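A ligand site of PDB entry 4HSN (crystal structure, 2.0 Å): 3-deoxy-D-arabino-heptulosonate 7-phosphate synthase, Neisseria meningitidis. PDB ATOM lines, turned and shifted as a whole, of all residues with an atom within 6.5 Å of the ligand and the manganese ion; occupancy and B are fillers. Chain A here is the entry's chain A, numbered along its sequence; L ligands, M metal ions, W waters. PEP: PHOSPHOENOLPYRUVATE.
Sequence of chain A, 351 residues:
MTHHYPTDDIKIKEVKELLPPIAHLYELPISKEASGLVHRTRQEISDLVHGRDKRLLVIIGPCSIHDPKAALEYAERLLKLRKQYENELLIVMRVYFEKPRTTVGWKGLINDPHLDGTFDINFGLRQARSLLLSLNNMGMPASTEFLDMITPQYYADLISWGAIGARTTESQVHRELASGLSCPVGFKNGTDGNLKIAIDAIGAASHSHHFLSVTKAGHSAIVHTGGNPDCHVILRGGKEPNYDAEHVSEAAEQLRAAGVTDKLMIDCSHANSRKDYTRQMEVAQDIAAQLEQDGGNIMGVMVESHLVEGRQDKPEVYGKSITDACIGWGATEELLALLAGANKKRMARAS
The side-chain amino group (NZ) of Lys 99 is in salt-bridge range of an oxygen (O2') of the ligand (3.1 Å). The side-chain amino group of Lys 188 is in salt-bridge range of an oxygen (O1) of the ligand, at 3.0 Å. An oxygen (O3P) of the ligand lies within salt-bridge range of the guanidinium group (NH1) of Arg 167, 2.9 Å away. An oxygen (O2') of the ligand sits close to a ring nitrogen (NE2) of His 270 (3.3 Å). An oxygen (O1P) of the ligand is in hydrogen-bond range of the backbone NH (N) of Ala 166, at 2.9 Å. The guanidinium group of Arg 94 is in salt-bridge range of an oxygen (O2') of the ligand (2.8 Å). The guanidinium group (NE) of Arg 236 lies within salt-bridge range of an oxygen (O2P) of the ligand (2.8 Å).
NE of Arg 94 lies within hydrogen-bond range of O of Pro 62, 2.9 Å away. N of Arg 236 sits at hydrogen-bond distance from OD1 of Asn 189 (2.8 Å). The side-chain sulfur of Cys 63 sits close to the side-chain hydroxyl of Thr 323 (2.9 Å). O of Cys 63 is in hydrogen-bond range of NH2 of Arg 94, 2.9 Å away. O of Thr 191 lies within hydrogen-bond range of NH2 of Arg 236. The side-chain carboxylate of Asp 267 is in salt-bridge range of the side-chain amino group of Lys 188 (3.0 Å). The backbone NH (N) of Lys 188 sits at hydrogen-bond distance from the backbone carbonyl oxygen (O) of Ile 164. OG of Ser 269 is in hydrogen-bond range of OE1 of Glu 304 (2.7 Å).
Tyr 96 touches the ligand (CE2 to O1, 3.6 Å). Glu 145 touches the ligand (OE1 to C3, 3.6 Å). Gly 165 touches the ligand. SD of Met 302 touches O1 of the ligand, 3.9 Å away. Hydrophobic or aromatic side chains within 4 Å of the ligand: Tyr 96, Ala 166, His 270 and Met 302.
Four residues have an atom within 4 Å of the manganese ion: Cys 63, His 270, Glu 304 and Asp 324. The nearest printed residue that does not touch the manganese ion is Lys 99 (4.1 Å).
The manganese ion is bound by water W1 (1.9 Å), the side-chain carboxylate of Asp 324 (2.0 Å), the side-chain carboxylate of Glu 304 (2.1 Å), a ring nitrogen (NE2) of His 270 (2.3 Å) and the side-chain sulfur of Cys 63 (2.7 Å). The manganese ion has five donor atoms within binding distance.
Water W2 lies within hydrogen-bond range of an oxygen (O1P) of the ligand (2.8 Å), the guanidinium group of Arg 167 (2.8 Å) and the backbone NH of Ala 166 (3.1 Å). Water W3 lies within hydrogen-bond range of OE1 of Glu 145 (2.6 Å) and O2 of the ligand (3.1 Å).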
ATOM      1  N   PRO A  62     -11.347 -12.533 -11.222  1.00  0.00           N
ATOM      2  CA  PRO A  62     -11.851 -13.089  -9.912  1.00  0.00           C
ATOM      3  C   PRO A  62     -12.061 -14.591  -9.861  1.00  0.00           C
ATOM      4  O   PRO A  62     -12.324 -15.197 -10.879  1.00  0.00           O
ATOM      5  CB  PRO A  62     -13.125 -12.301  -9.692  1.00  0.00           C
ATOM      6  CG  PRO A  62     -12.945 -11.028 -10.373  1.00  0.00           C
ATOM      7  CD  PRO A  62     -12.184 -11.431 -11.672  1.00  0.00           C
ATOM      8  N   CYS A  63     -11.817 -15.184  -8.716  1.00  0.00           N
ATOM      9  CA  CYS A  63     -12.165 -16.554  -8.521  1.00  0.00           C
ATOM     10  C   CYS A  63     -13.718 -16.631  -8.866  1.00  0.00           C
ATOM     11  O   CYS A  63     -14.117 -17.507  -9.626  1.00  0.00           O
ATOM     12  CB  CYS A  63     -11.909 -16.925  -7.079  1.00  0.00           C
ATOM     13  SG  CYS A  63     -12.504 -18.580  -6.602  1.00  0.00           S
ATOM     14  N   SER A  64     -14.483 -15.714  -8.323  1.00  0.00           N
ATOM     15  CA  SER A  64     -15.901 -15.698  -8.523  1.00  0.00           C
ATOM     16  C   SER A  64     -16.409 -14.282  -8.623  1.00  0.00           C
ATOM     17  O   SER A  64     -15.845 -13.369  -8.019  1.00  0.00           O
ATOM     18  CB  SER A  64     -16.567 -16.354  -7.341  1.00  0.00           C
ATOM     19  OG  SER A  64     -16.285 -15.694  -6.101  1.00  0.00           O
ATOM     20  N   ARG A  94     -11.893 -13.711 -16.475  1.00  0.00           N
ATOM     21  CA  ARG A  94     -12.600 -14.740 -15.712  1.00  0.00           C
ATOM     22  C   ARG A  94     -13.887 -14.121 -15.189  1.00  0.00           C
ATOM     23  O   ARG A  94     -13.852 -13.132 -14.414  1.00  0.00           O
ATOM     24  CB  ARG A  94     -11.840 -15.194 -14.445  1.00  0.00           C
ATOM     25  CG  ARG A  94     -10.641 -16.110 -14.717  1.00  0.00           C
ATOM     26  CD  ARG A  94      -9.938 -16.535 -13.440  1.00  0.00           C
ATOM     27  NE  ARG A  94     -10.878 -17.107 -12.496  1.00  0.00           N
ATOM     28  CZ  ARG A  94     -10.994 -18.370 -12.101  1.00  0.00           C
ATOM     29  NH1 ARG A  94     -10.290 -19.312 -12.595  1.00  0.00           N
ATOM     30  NH2 ARG A  94     -11.975 -18.687 -11.243  1.00  0.00           N
ATOM     31  N   TYR A  96     -16.793 -16.031 -13.538  1.00  0.00           N
ATOM     32  CA  TYR A  96     -17.238 -17.313 -13.068  1.00  0.00           C
ATOM     33  C   TYR A  96     -18.465 -17.151 -12.171  1.00  0.00           C
ATOM     34  O   TYR A  96     -18.360 -16.492 -11.138  1.00  0.00           O
ATOM     35  CB  TYR A  96     -16.108 -17.950 -12.303  1.00  0.00           C
ATOM     36  CG  TYR A  96     -15.106 -18.679 -13.156  1.00  0.00           C
ATOM     37  CD1 TYR A  96     -14.505 -18.079 -14.261  1.00  0.00           C
ATOM     38  CD2 TYR A  96     -14.696 -19.943 -12.838  1.00  0.00           C
ATOM     39  CE1 TYR A  96     -13.561 -18.763 -15.048  1.00  0.00           C
ATOM     40  CE2 TYR A  96     -13.690 -20.622 -13.540  1.00  0.00           C
ATOM     41  CZ  TYR A  96     -13.131 -20.005 -14.650  1.00  0.00           C
ATOM     42  OH  TYR A  96     -12.192 -20.731 -15.408  1.00  0.00           O
ATOM     43  N   GLU A  98     -20.507 -19.884 -11.339  1.00  0.00           N
ATOM     44  CA  GLU A  98     -20.809 -21.206 -10.719  1.00  0.00           C
ATOM     45  C   GLU A  98     -19.560 -21.762 -10.069  1.00  0.00           C
ATOM     46  O   GLU A  98     -18.544 -21.936 -10.770  1.00  0.00           O
ATOM     47  CB  GLU A  98     -21.294 -22.171 -11.789  1.00  0.00           C
ATOM     48  CG  GLU A  98     -22.461 -21.637 -12.596  1.00  0.00           C
ATOM     49  CD  GLU A  98     -23.099 -22.625 -13.607  1.00  0.00           C
ATOM     50  OE1 GLU A  98     -22.435 -23.513 -14.209  1.00  0.00           O
ATOM     51  OE2 GLU A  98     -24.273 -22.316 -13.886  1.00  0.00           O
ATOM     52  N   LYS A  99     -19.633 -22.056  -8.776  1.00  0.00           N
ATOM     53  CA  LYS A  99     -18.498 -22.504  -7.970  1.00  0.00           C
ATOM     54  C   LYS A  99     -18.794 -23.863  -7.410  1.00  0.00           C
ATOM     55  O   LYS A  99     -19.741 -24.036  -6.663  1.00  0.00           O
ATOM     56  CB  LYS A  99     -18.197 -21.506  -6.826  1.00  0.00           C
ATOM     57  CG  LYS A  99     -18.017 -20.066  -7.286  1.00  0.00           C
ATOM     58  CD  LYS A  99     -16.946 -19.967  -8.421  1.00  0.00           C
ATOM     59  CE  LYS A  99     -15.550 -20.369  -7.833  1.00  0.00           C
ATOM     60  NZ  LYS A  99     -14.542 -20.424  -8.942  1.00  0.00           N
ATOM     61  N   PRO A 100     -17.878 -24.832  -7.648  1.00  0.00           N
ATOM     62  CA  PRO A 100     -18.035 -26.122  -7.052  1.00  0.00           C
ATOM     63  C   PRO A 100     -17.439 -26.074  -5.665  1.00  0.00           C
ATOM     64  O   PRO A 100     -16.315 -25.599  -5.505  1.00  0.00           O
ATOM     65  CB  PRO A 100     -17.197 -27.026  -7.977  1.00  0.00           C
ATOM     66  CG  PRO A 100     -16.118 -26.124  -8.538  1.00  0.00           C
ATOM     67  CD  PRO A 100     -16.772 -24.767  -8.639  1.00  0.00           C
ATOM     68  N   GLU A 145     -16.570 -21.180 -15.884  1.00  0.00           N
ATOM     69  CA  GLU A 145     -16.705 -22.579 -15.710  1.00  0.00           C
ATOM     70  C   GLU A 145     -18.076 -23.013 -15.954  1.00  0.00           C
ATOM     71  O   GLU A 145     -18.994 -22.451 -15.357  1.00  0.00           O
ATOM     72  CB  GLU A 145     -16.292 -23.050 -14.331  1.00  0.00           C
ATOM     73  CG  GLU A 145     -16.460 -24.578 -14.117  1.00  0.00           C
ATOM     74  CD  GLU A 145     -16.082 -25.174 -12.762  1.00  0.00           C
ATOM     75  OE1 GLU A 145     -15.249 -24.552 -12.014  1.00  0.00           O
ATOM     76  OE2 GLU A 145     -16.550 -26.348 -12.495  1.00  0.00           O
ATOM     77  N   ALA A 163     -14.194 -23.401 -19.026  1.00  0.00           N
ATOM     78  CA  ALA A 163     -13.489 -24.411 -18.279  1.00  0.00           C
ATOM     79  C   ALA A 163     -14.391 -25.455 -17.803  1.00  0.00           C
ATOM     80  O   ALA A 163     -15.599 -25.199 -17.474  1.00  0.00           O
ATOM     81  CB  ALA A 163     -12.788 -23.827 -17.122  1.00  0.00           C
ATOM     82  N   ILE A 164     -13.866 -26.688 -17.752  1.00  0.00           N
ATOM     83  CA  ILE A 164     -14.512 -27.736 -16.989  1.00  0.00           C
ATOM     84  C   ILE A 164     -13.630 -27.979 -15.814  1.00  0.00           C
ATOM     85  O   ILE A 164     -12.403 -28.218 -15.967  1.00  0.00           O
ATOM     86  CB  ILE A 164     -14.694 -29.025 -17.803  1.00  0.00           C
ATOM     87  CG1 ILE A 164     -15.625 -28.764 -19.003  1.00  0.00           C
ATOM     88  CG2 ILE A 164     -15.277 -30.134 -16.866  1.00  0.00           C
ATOM     89  CD1 ILE A 164     -17.081 -28.423 -18.657  1.00  0.00           C
ATOM     90  N   GLY A 165     -14.194 -27.911 -14.626  1.00  0.00           N
ATOM     91  CA  GLY A 165     -13.436 -27.997 -13.403  1.00  0.00           C
ATOM     92  C   GLY A 165     -12.731 -29.325 -13.072  1.00  0.00           C
ATOM     93  O   GLY A 165     -13.090 -30.395 -13.581  1.00  0.00           O
ATOM     94  N   ALA A 166     -11.824 -29.272 -12.147  1.00  0.00           N
ATOM     95  CA  ALA A 166     -11.060 -30.477 -11.811  1.00  0.00           C
ATOM     96  C   ALA A 166     -11.969 -31.574 -11.275  1.00  0.00           C
ATOM     97  O   ALA A 166     -11.764 -32.773 -11.517  1.00  0.00           O
ATOM     98  CB  ALA A 166      -9.936 -30.127 -10.797  1.00  0.00           C
ATOM     99  N   ARG A 167     -13.042 -31.178 -10.604  1.00  0.00           N
ATOM    100  CA  ARG A 167     -13.945 -32.079  -9.963  1.00  0.00           C
ATOM    101  C   ARG A 167     -14.925 -32.715 -10.950  1.00  0.00           C
ATOM    102  O   ARG A 167     -15.677 -33.582 -10.566  1.00  0.00           O
ATOM    103  CB  ARG A 167     -14.706 -31.352  -8.839  1.00  0.00           C
ATOM    104  CG  ARG A 167     -13.766 -30.932  -7.704  1.00  0.00           C
ATOM    105  CD  ARG A 167     -14.416 -29.991  -6.678  1.00  0.00           C
ATOM    106  NE  ARG A 167     -13.420 -29.434  -5.768  1.00  0.00           N
ATOM    107  CZ  ARG A 167     -12.501 -28.506  -6.062  1.00  0.00           C
ATOM    108  NH1 ARG A 167     -12.369 -27.983  -7.264  1.00  0.00           N
ATOM    109  NH2 ARG A 167     -11.596 -28.158  -5.156  1.00  0.00           N
ATOM    110  N   LYS A 188      -9.462 -29.306 -16.714  1.00  0.00           N
ATOM    111  CA  LYS A 188      -8.469 -29.355 -15.658  1.00  0.00           C
ATOM    112  C   LYS A 188      -8.144 -30.743 -15.263  1.00  0.00           C
ATOM    113  O   LYS A 188      -9.010 -31.648 -15.291  1.00  0.00           O
ATOM    114  CB  LYS A 188      -9.012 -28.604 -14.434  1.00  0.00           C
ATOM    115  CG  LYS A 188      -9.128 -27.121 -14.719  1.00  0.00           C
ATOM    116  CD  LYS A 188      -9.356 -26.294 -13.505  1.00  0.00           C
ATOM    117  CE  LYS A 188      -8.541 -24.986 -13.648  1.00  0.00           C
ATOM    118  NZ  LYS A 188      -8.760 -24.204 -12.390  1.00  0.00           N
ATOM    119  N   ASN A 189      -6.871 -30.970 -14.912  1.00  0.00           N
ATOM    120  CA  ASN A 189      -6.493 -32.206 -14.326  1.00  0.00           C
ATOM    121  C   ASN A 189      -7.186 -32.413 -12.979  1.00  0.00           C
ATOM    122  O   ASN A 189      -7.787 -31.441 -12.409  1.00  0.00           O
ATOM    123  CB  ASN A 189      -4.905 -32.363 -14.198  1.00  0.00           C
ATOM    124  CG  ASN A 189      -4.273 -31.394 -13.197  1.00  0.00           C
ATOM    125  OD1 ASN A 189      -3.590 -30.458 -13.561  1.00  0.00           O
ATOM    126  ND2 ASN A 189      -4.574 -31.564 -11.900  1.00  0.00           N
ATOM    127  N   THR A 191      -8.180 -33.393  -8.962  1.00  0.00           N
ATOM    128  CA  THR A 191      -7.780 -32.685  -7.798  1.00  0.00           C
ATOM    129  C   THR A 191      -6.549 -33.260  -7.133  1.00  0.00           C
ATOM    130  O   THR A 191      -5.847 -32.525  -6.435  1.00  0.00           O
ATOM    131  CB  THR A 191      -8.939 -32.592  -6.772  1.00  0.00           C
ATOM    132  OG1 THR A 191      -9.473 -33.905  -6.552  1.00  0.00           O
ATOM    133  CG2 THR A 191     -10.021 -31.653  -7.287  1.00  0.00           C
ATOM    134  N   ARG A 236      -3.267 -27.686 -13.148  1.00  0.00           N
ATOM    135  CA  ARG A 236      -3.642 -26.906 -11.976  1.00  0.00           C
ATOM    136  C   ARG A 236      -3.206 -27.455 -10.687  1.00  0.00           C
ATOM    137  O   ARG A 236      -3.737 -27.082  -9.604  1.00  0.00           O
ATOM    138  CB  ARG A 236      -5.222 -26.670 -11.918  1.00  0.00           C
ATOM    139  CG  ARG A 236      -6.067 -27.871 -12.123  1.00  0.00           C
ATOM    140  CD  ARG A 236      -6.175 -28.734 -10.882  1.00  0.00           C
ATOM    141  NE  ARG A 236      -6.933 -28.115  -9.803  1.00  0.00           N
ATOM    142  CZ  ARG A 236      -6.936 -28.499  -8.521  1.00  0.00           C
ATOM    143  NH1 ARG A 236      -7.717 -27.885  -7.636  1.00  0.00           N
ATOM    144  NH2 ARG A 236      -6.236 -29.529  -8.093  1.00  0.00           N
ATOM    145  N   ASP A 267      -2.368 -23.212 -14.873  1.00  0.00           N
ATOM    146  CA  ASP A 267      -3.090 -22.394 -13.826  1.00  0.00           C
ATOM    147  C   ASP A 267      -2.111 -22.006 -12.750  1.00  0.00           C
ATOM    148  O   ASP A 267      -1.463 -22.895 -12.183  1.00  0.00           O
ATOM    149  CB  ASP A 267      -4.214 -23.251 -13.225  1.00  0.00           C
ATOM    150  CG  ASP A 267      -5.092 -22.469 -12.215  1.00  0.00           C
ATOM    151  OD1 ASP A 267      -4.826 -21.280 -11.927  1.00  0.00           O
ATOM    152  OD2 ASP A 267      -6.093 -23.069 -11.784  1.00  0.00           O
ATOM    153  N   SER A 269      -2.874 -20.628 -10.062  1.00  0.00           N
ATOM    154  CA  SER A 269      -3.598 -20.565  -8.748  1.00  0.00           C
ATOM    155  C   SER A 269      -3.922 -21.988  -8.249  1.00  0.00           C
ATOM    156  O   SER A 269      -3.225 -22.987  -8.620  1.00  0.00           O
ATOM    157  CB  SER A 269      -4.840 -19.671  -8.845  1.00  0.00           C
ATOM    158  OG  SER A 269      -5.313 -19.280  -7.536  1.00  0.00           O
ATOM    159  N   HIS A 270      -4.917 -22.074  -7.329  1.00  0.00           N
ATOM    160  CA  HIS A 270      -5.338 -23.369  -6.848  1.00  0.00           C
ATOM    161  C   HIS A 270      -4.165 -24.248  -6.367  1.00  0.00           C
ATOM    162  O   HIS A 270      -3.363 -23.800  -5.522  1.00  0.00           O
ATOM    163  CB  HIS A 270      -6.265 -24.040  -7.888  1.00  0.00           C
ATOM    164  CG  HIS A 270      -7.403 -23.142  -8.272  1.00  0.00           C
ATOM    165  ND1 HIS A 270      -7.478 -22.507  -9.500  1.00  0.00           N
ATOM    166  CD2 HIS A 270      -8.484 -22.697  -7.551  1.00  0.00           C
ATOM    167  CE1 HIS A 270      -8.506 -21.660  -9.482  1.00  0.00           C
ATOM    168  NE2 HIS A 270      -9.129 -21.795  -8.330  1.00  0.00           N
ATOM    169  N   ALA A 271      -4.064 -25.480  -6.811  1.00  0.00           N
ATOM    170  CA  ALA A 271      -3.044 -26.383  -6.241  1.00  0.00           C
ATOM    171  C   ALA A 271      -1.621 -26.111  -6.751  1.00  0.00           C
ATOM    172  O   ALA A 271      -0.666 -26.619  -6.200  1.00  0.00           O
ATOM    173  CB  ALA A 271      -3.428 -27.833  -6.434  1.00  0.00           C
ATOM    174  N   MET A 302      -3.619 -19.204 -16.464  1.00  0.00           N
ATOM    175  CA  MET A 302      -4.765 -18.783 -15.703  1.00  0.00           C
ATOM    176  C   MET A 302      -4.356 -18.155 -14.392  1.00  0.00           C
ATOM    177  O   MET A 302      -3.416 -18.616 -13.746  1.00  0.00           O
ATOM    178  CB  MET A 302      -5.762 -19.983 -15.572  1.00  0.00           C
ATOM    179  CG  MET A 302      -6.828 -19.751 -14.541  1.00  0.00           C
ATOM    180  SD  MET A 302      -8.041 -21.149 -14.319  1.00  0.00           S
ATOM    181  CE  MET A 302      -8.324 -21.598 -16.011  1.00  0.00           C
ATOM    182  N   GLU A 304      -5.913 -15.918 -10.818  1.00  0.00           N
ATOM    183  CA  GLU A 304      -7.029 -15.365  -9.957  1.00  0.00           C
ATOM    184  C   GLU A 304      -6.601 -14.039  -9.337  1.00  0.00           C
ATOM    185  O   GLU A 304      -5.571 -13.928  -8.636  1.00  0.00           O
ATOM    186  CB  GLU A 304      -7.402 -16.348  -8.917  1.00  0.00           C
ATOM    187  CG  GLU A 304      -8.046 -17.574  -9.519  1.00  0.00           C
ATOM    188  CD  GLU A 304      -8.680 -18.490  -8.460  1.00  0.00           C
ATOM    189  OE1 GLU A 304      -8.010 -18.843  -7.460  1.00  0.00           O
ATOM    190  OE2 GLU A 304      -9.869 -18.860  -8.693  1.00  0.00           O
ATOM    191  N   THR A 323     -14.460 -15.864  -2.316  1.00  0.00           N
ATOM    192  CA  THR A 323     -14.096 -17.293  -2.477  1.00  0.00           C
ATOM    193  C   THR A 323     -12.527 -17.458  -2.343  1.00  0.00           C
ATOM    194  O   THR A 323     -11.991 -17.085  -1.314  1.00  0.00           O
ATOM    195  CB  THR A 323     -14.699 -17.943  -3.790  1.00  0.00           C
ATOM    196  OG1 THR A 323     -14.439 -17.118  -4.948  1.00  0.00           O
ATOM    197  CG2 THR A 323     -16.254 -18.166  -3.591  1.00  0.00           C
ATOM    198  N   ASP A 324     -11.824 -18.015  -3.323  1.00  0.00           N
ATOM    199  CA  ASP A 324     -10.328 -18.149  -3.194  1.00  0.00           C
ATOM    200  C   ASP A 324      -9.706 -16.743  -3.157  1.00  0.00           C
ATOM    201  O   ASP A 324     -10.145 -15.837  -3.834  1.00  0.00           O
ATOM    202  CB  ASP A 324      -9.661 -18.940  -4.379  1.00  0.00           C
ATOM    203  CG  ASP A 324     -10.168 -20.388  -4.500  1.00  0.00           C
ATOM    204  OD1 ASP A 324     -10.629 -20.939  -3.531  1.00  0.00           O
ATOM    205  OD2 ASP A 324     -10.298 -20.843  -5.650  1.00  0.00           O
HETATM  206  C1  PEP L   1     -11.467 -22.265 -10.737  1.00  0.00           C
HETATM  207  O1  PEP L   1     -10.875 -22.149 -11.849  1.00  0.00           O
HETATM  208  O2' PEP L   1     -11.855 -21.266 -10.118  1.00  0.00           O
HETATM  209  C2  PEP L   1     -11.734 -23.611 -10.131  1.00  0.00           C
HETATM  210  C3  PEP L   1     -12.858 -23.896  -9.456  1.00  0.00           C
HETATM  211  O2  PEP L   1     -10.753 -24.637 -10.408  1.00  0.00           O
HETATM  212  P   PEP L   1     -10.422 -26.079  -9.819  1.00  0.00           P
HETATM  213  O1P PEP L   1     -11.446 -26.809 -10.654  1.00  0.00           O
HETATM  214  O2P PEP L   1      -8.900 -26.131 -10.081  1.00  0.00           O
HETATM  215  O3P PEP L   1     -10.575 -26.030  -8.324  1.00  0.00           O
HETATM  216 MN    MN M   1     -10.705 -20.333  -7.492  1.00  0.00          MN
HETATM  217  O   HOH W   1     -12.098 -21.602  -7.779  1.00  0.00           O
HETATM  218  O   HOH W   2     -13.647 -28.368  -9.777  1.00  0.00           O
HETATM  219  O   HOH W   3     -12.751 -24.634 -12.768  1.00  0.00           O
